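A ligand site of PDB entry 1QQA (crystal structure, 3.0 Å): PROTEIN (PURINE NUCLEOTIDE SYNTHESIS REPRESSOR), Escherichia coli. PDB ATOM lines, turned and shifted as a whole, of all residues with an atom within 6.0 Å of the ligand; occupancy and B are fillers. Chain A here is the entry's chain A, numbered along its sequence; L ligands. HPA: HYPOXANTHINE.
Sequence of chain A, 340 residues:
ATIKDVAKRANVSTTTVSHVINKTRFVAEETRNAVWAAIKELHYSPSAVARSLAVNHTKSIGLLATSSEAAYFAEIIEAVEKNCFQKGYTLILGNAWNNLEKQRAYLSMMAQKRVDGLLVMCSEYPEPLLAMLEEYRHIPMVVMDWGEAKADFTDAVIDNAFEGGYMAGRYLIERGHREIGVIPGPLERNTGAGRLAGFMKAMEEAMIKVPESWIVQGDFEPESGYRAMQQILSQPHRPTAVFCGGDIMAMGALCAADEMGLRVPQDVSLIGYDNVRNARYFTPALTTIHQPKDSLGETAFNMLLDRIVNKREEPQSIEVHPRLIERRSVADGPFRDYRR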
ATOM      1  N   ALA A  70      -7.197  23.285  19.974  1.00  0.00           N
ATOM      2  CA  ALA A  70      -5.776  23.291  20.104  1.00  0.00           C
ATOM      3  C   ALA A  70      -5.000  22.362  19.207  1.00  0.00           C
ATOM      4  O   ALA A  70      -5.180  21.139  19.188  1.00  0.00           O
ATOM      5  CB  ALA A  70      -5.444  22.955  21.510  1.00  0.00           C
ATOM      6  N   TYR A  72      -2.256  21.014  19.335  1.00  0.00           N
ATOM      7  CA  TYR A  72      -1.726  19.845  19.945  1.00  0.00           C
ATOM      8  C   TYR A  72      -2.775  18.757  19.995  1.00  0.00           C
ATOM      9  O   TYR A  72      -2.579  17.613  19.578  1.00  0.00           O
ATOM     10  CB  TYR A  72      -1.186  20.226  21.335  1.00  0.00           C
ATOM     11  CG  TYR A  72      -0.589  19.083  22.105  1.00  0.00           C
ATOM     12  CD1 TYR A  72       0.617  18.545  21.731  1.00  0.00           C
ATOM     13  CD2 TYR A  72      -1.226  18.555  23.216  1.00  0.00           C
ATOM     14  CE1 TYR A  72       1.198  17.490  22.436  1.00  0.00           C
ATOM     15  CE2 TYR A  72      -0.667  17.521  23.922  1.00  0.00           C
ATOM     16  CZ  TYR A  72       0.541  16.986  23.508  1.00  0.00           C
ATOM     17  OH  TYR A  72       1.112  15.941  24.152  1.00  0.00           O
ATOM     18  N   PHE A  73      -3.925  19.158  20.513  1.00  0.00           N
ATOM     19  CA  PHE A  73      -4.986  18.233  20.664  1.00  0.00           C
ATOM     20  C   PHE A  73      -5.513  17.729  19.413  1.00  0.00           C
ATOM     21  O   PHE A  73      -5.673  16.516  19.147  1.00  0.00           O
ATOM     22  CB  PHE A  73      -6.110  18.913  21.399  1.00  0.00           C
ATOM     23  CG  PHE A  73      -5.792  19.083  22.839  1.00  0.00           C
ATOM     24  CD1 PHE A  73      -4.779  18.358  23.372  1.00  0.00           C
ATOM     25  CD2 PHE A  73      -6.429  20.018  23.613  1.00  0.00           C
ATOM     26  CE1 PHE A  73      -4.476  18.509  24.663  1.00  0.00           C
ATOM     27  CE2 PHE A  73      -6.093  20.172  24.940  1.00  0.00           C
ATOM     28  CZ  PHE A  73      -5.084  19.473  25.440  1.00  0.00           C
ATOM     29  N   SER A 123      -6.053  16.127  30.889  1.00  0.00           N
ATOM     30  CA  SER A 123      -5.093  17.172  31.200  1.00  0.00           C
ATOM     31  C   SER A 123      -4.839  17.222  32.649  1.00  0.00           C
ATOM     32  O   SER A 123      -3.750  16.948  33.054  1.00  0.00           O
ATOM     33  CB  SER A 123      -5.517  18.540  30.671  1.00  0.00           C
ATOM     34  OG  SER A 123      -5.585  18.460  29.267  1.00  0.00           O
ATOM     35  N   PRO A 186       0.707  24.850  32.484  1.00  0.00           N
ATOM     36  CA  PRO A 186       0.111  24.572  33.803  1.00  0.00           C
ATOM     37  C   PRO A 186       0.815  23.452  34.576  1.00  0.00           C
ATOM     38  O   PRO A 186       0.996  22.356  34.056  1.00  0.00           O
ATOM     39  CB  PRO A 186      -1.309  24.202  33.458  1.00  0.00           C
ATOM     40  CG  PRO A 186      -1.542  24.828  32.126  1.00  0.00           C
ATOM     41  CD  PRO A 186      -0.256  24.619  31.410  1.00  0.00           C
ATOM     42  N   ARG A 189      -0.335  19.731  35.080  1.00  0.00           N
ATOM     43  CA  ARG A 189      -0.278  18.883  33.921  1.00  0.00           C
ATOM     44  C   ARG A 189       1.090  18.291  33.761  1.00  0.00           C
ATOM     45  O   ARG A 189       2.048  18.781  34.318  1.00  0.00           O
ATOM     46  CB  ARG A 189      -0.542  19.724  32.708  1.00  0.00           C
ATOM     47  CG  ARG A 189      -1.948  19.630  32.258  1.00  0.00           C
ATOM     48  CD  ARG A 189      -2.532  20.974  32.180  1.00  0.00           C
ATOM     49  NE  ARG A 189      -2.958  21.172  30.819  1.00  0.00           N
ATOM     50  CZ  ARG A 189      -4.050  21.844  30.526  1.00  0.00           C
ATOM     51  NH1 ARG A 189      -4.748  22.363  31.524  1.00  0.00           N
ATOM     52  NH2 ARG A 189      -4.425  22.027  29.260  1.00  0.00           N
ATOM     53  N   THR A 191       2.658  17.715  30.658  1.00  0.00           N
ATOM     54  CA  THR A 191       3.254  18.564  29.650  1.00  0.00           C
ATOM     55  C   THR A 191       3.638  19.876  30.260  1.00  0.00           C
ATOM     56  O   THR A 191       4.466  20.572  29.655  1.00  0.00           O
ATOM     57  CB  THR A 191       2.334  18.807  28.471  1.00  0.00           C
ATOM     58  OG1 THR A 191       1.027  19.069  28.952  1.00  0.00           O
ATOM     59  CG2 THR A 191       2.299  17.612  27.515  1.00  0.00           C
ATOM     60  N   GLY A 192       3.059  20.218  31.436  1.00  0.00           N
ATOM     61  CA  GLY A 192       3.380  21.442  32.205  1.00  0.00           C
ATOM     62  C   GLY A 192       4.572  21.048  33.152  1.00  0.00           C
ATOM     63  O   GLY A 192       5.767  21.116  32.824  1.00  0.00           O
ATOM     64  N   ARG A 195       7.768  18.919  31.933  1.00  0.00           N
ATOM     65  CA  ARG A 195       8.689  19.425  30.953  1.00  0.00           C
ATOM     66  C   ARG A 195       9.647  20.335  31.732  1.00  0.00           C
ATOM     67  O   ARG A 195      10.886  20.245  31.653  1.00  0.00           O
ATOM     68  CB  ARG A 195       7.922  20.074  29.781  1.00  0.00           C
ATOM     69  CG  ARG A 195       7.341  19.079  28.709  1.00  0.00           C
ATOM     70  CD  ARG A 195       6.365  19.790  27.715  1.00  0.00           C
ATOM     71  NE  ARG A 195       5.609  18.920  26.802  1.00  0.00           N
ATOM     72  CZ  ARG A 195       4.826  19.371  25.819  1.00  0.00           C
ATOM     73  NH1 ARG A 195       4.711  20.671  25.583  1.00  0.00           N
ATOM     74  NH2 ARG A 195       4.151  18.528  25.064  1.00  0.00           N
ATOM     75  N   ASP A 219      -0.551  28.985  29.836  1.00  0.00           N
ATOM     76  CA  ASP A 219      -1.703  28.074  29.908  1.00  0.00           C
ATOM     77  C   ASP A 219      -1.836  27.403  28.571  1.00  0.00           C
ATOM     78  O   ASP A 219      -2.942  27.010  28.170  1.00  0.00           O
ATOM     79  CB  ASP A 219      -2.961  28.912  30.124  1.00  0.00           C
ATOM     80  CG  ASP A 219      -3.193  29.932  29.024  1.00  0.00           C
ATOM     81  OD1 ASP A 219      -2.423  30.047  28.057  1.00  0.00           O
ATOM     82  OD2 ASP A 219      -4.182  30.650  29.128  1.00  0.00           O
ATOM     83  N   PHE A 220      -0.728  27.328  27.862  1.00  0.00           N
ATOM     84  CA  PHE A 220      -0.628  26.762  26.501  1.00  0.00           C
ATOM     85  C   PHE A 220      -1.269  27.602  25.396  1.00  0.00           C
ATOM     86  O   PHE A 220      -1.315  27.173  24.250  1.00  0.00           O
ATOM     87  CB  PHE A 220      -1.177  25.362  26.409  1.00  0.00           C
ATOM     88  CG  PHE A 220      -0.266  24.324  26.941  1.00  0.00           C
ATOM     89  CD1 PHE A 220       0.979  24.147  26.382  1.00  0.00           C
ATOM     90  CD2 PHE A 220      -0.644  23.531  28.014  1.00  0.00           C
ATOM     91  CE1 PHE A 220       1.836  23.170  26.877  1.00  0.00           C
ATOM     92  CE2 PHE A 220       0.184  22.582  28.511  1.00  0.00           C
ATOM     93  CZ  PHE A 220       1.435  22.398  27.941  1.00  0.00           C
ATOM     94  N   GLY A 245       7.289  26.269  26.948  1.00  0.00           N
ATOM     95  CA  GLY A 245       6.485  25.071  27.203  1.00  0.00           C
ATOM     96  C   GLY A 245       5.806  24.306  26.087  1.00  0.00           C
ATOM     97  O   GLY A 245       5.774  23.088  26.106  1.00  0.00           O
ATOM     98  N   GLY A 246       5.229  25.030  25.134  1.00  0.00           N
ATOM     99  CA  GLY A 246       4.543  24.474  23.962  1.00  0.00           C
ATOM    100  C   GLY A 246       4.704  25.426  22.768  1.00  0.00           C
ATOM    101  O   GLY A 246       4.899  26.667  22.936  1.00  0.00           O
ATOM    102  N   TYR A 273       8.220  23.583  22.199  1.00  0.00           N
ATOM    103  CA  TYR A 273       7.983  22.220  22.564  1.00  0.00           C
ATOM    104  C   TYR A 273       6.680  21.739  22.048  1.00  0.00           C
ATOM    105  O   TYR A 273       5.649  22.263  22.497  1.00  0.00           O
ATOM    106  CB  TYR A 273       7.967  22.081  24.079  1.00  0.00           C
ATOM    107  CG  TYR A 273       8.241  20.646  24.474  1.00  0.00           C
ATOM    108  CD1 TYR A 273       7.530  19.597  23.913  1.00  0.00           C
ATOM    109  CD2 TYR A 273       9.250  20.340  25.391  1.00  0.00           C
ATOM    110  CE1 TYR A 273       7.807  18.294  24.277  1.00  0.00           C
ATOM    111  CE2 TYR A 273       9.519  19.043  25.746  1.00  0.00           C
ATOM    112  CZ  TYR A 273       8.810  18.025  25.202  1.00  0.00           C
ATOM    113  OH  TYR A 273       9.159  16.761  25.613  1.00  0.00           O
ATOM    114  N   ASP A 274       6.770  20.749  21.158  1.00  0.00           N
ATOM    115  CA  ASP A 274       5.608  20.061  20.535  1.00  0.00           C
ATOM    116  C   ASP A 274       5.804  19.612  19.100  1.00  0.00           C
ATOM    117  O   ASP A 274       5.454  18.501  18.712  1.00  0.00           O
ATOM    118  CB  ASP A 274       4.303  20.879  20.587  1.00  0.00           C
ATOM    119  CG  ASP A 274       3.558  20.749  21.907  1.00  0.00           C
ATOM    120  OD1 ASP A 274       4.058  20.065  22.828  1.00  0.00           O
ATOM    121  OD2 ASP A 274       2.558  21.465  22.083  1.00  0.00           O
HETATM  122  N1  HPA L   1      -2.733  21.923  25.827  1.00  0.00           N
HETATM  123  C2  HPA L   1      -2.334  22.421  24.613  1.00  0.00           C
HETATM  124  N3  HPA L   1      -1.188  22.134  24.016  1.00  0.00           N
HETATM  125  C4  HPA L   1      -0.423  21.303  24.756  1.00  0.00           C
HETATM  126  C5  HPA L   1      -0.720  20.750  25.981  1.00  0.00           C
HETATM  127  C6  HPA L   1      -1.963  21.052  26.601  1.00  0.00           C
HETATM  128  O6  HPA L   1      -2.448  20.663  27.668  1.00  0.00           O
HETATM  129  N7  HPA L   1       0.325  19.938  26.393  1.00  0.00           N
HETATM  130  C8  HPA L   1       1.219  20.005  25.442  1.00  0.00           C
HETATM  131  N9  HPA L   1       0.816  20.809  24.405  1.00  0.00           N
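The guanidinium group of Arg 195 lies within hydrogen-bond range of the backbone carbonyl oxygen of Gly 245. NH2 of Arg 195 is in salt-bridge range of OD1 of Asp 274 (2.7 Å). The backbone carbonyl oxygen of Thr 191 sits close to the guanidinium group of Arg 195.
A nitrogen (N7) of the ligand is in hydrogen-bond range of the side-chain hydroxyl of Thr 191 (2.8 Å). OD2 of Asp 274 sits close to N9 of the ligand, at 3.0 Å. The guanidinium group (NH2) of Arg 189 is in hydrogen-bond range of an oxygen (O6) of the ligand, 2.9 Å away.
Tyr 72 touches the ligand (CG to N9, 3.2 Å). Phe 73 touches the ligand (CZ to N1, 3.4 Å). Arg 195 touches the ligand (NH2 to C8, 3.3 Å). Phe 220 touches the ligand. Hydrophobic or aromatic side chains within 4 Å of the ligand: Tyr 72, Phe 73 and Phe 220. The nearest printed residue that does not touch the ligand is Ser 123 (4.2 Å).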
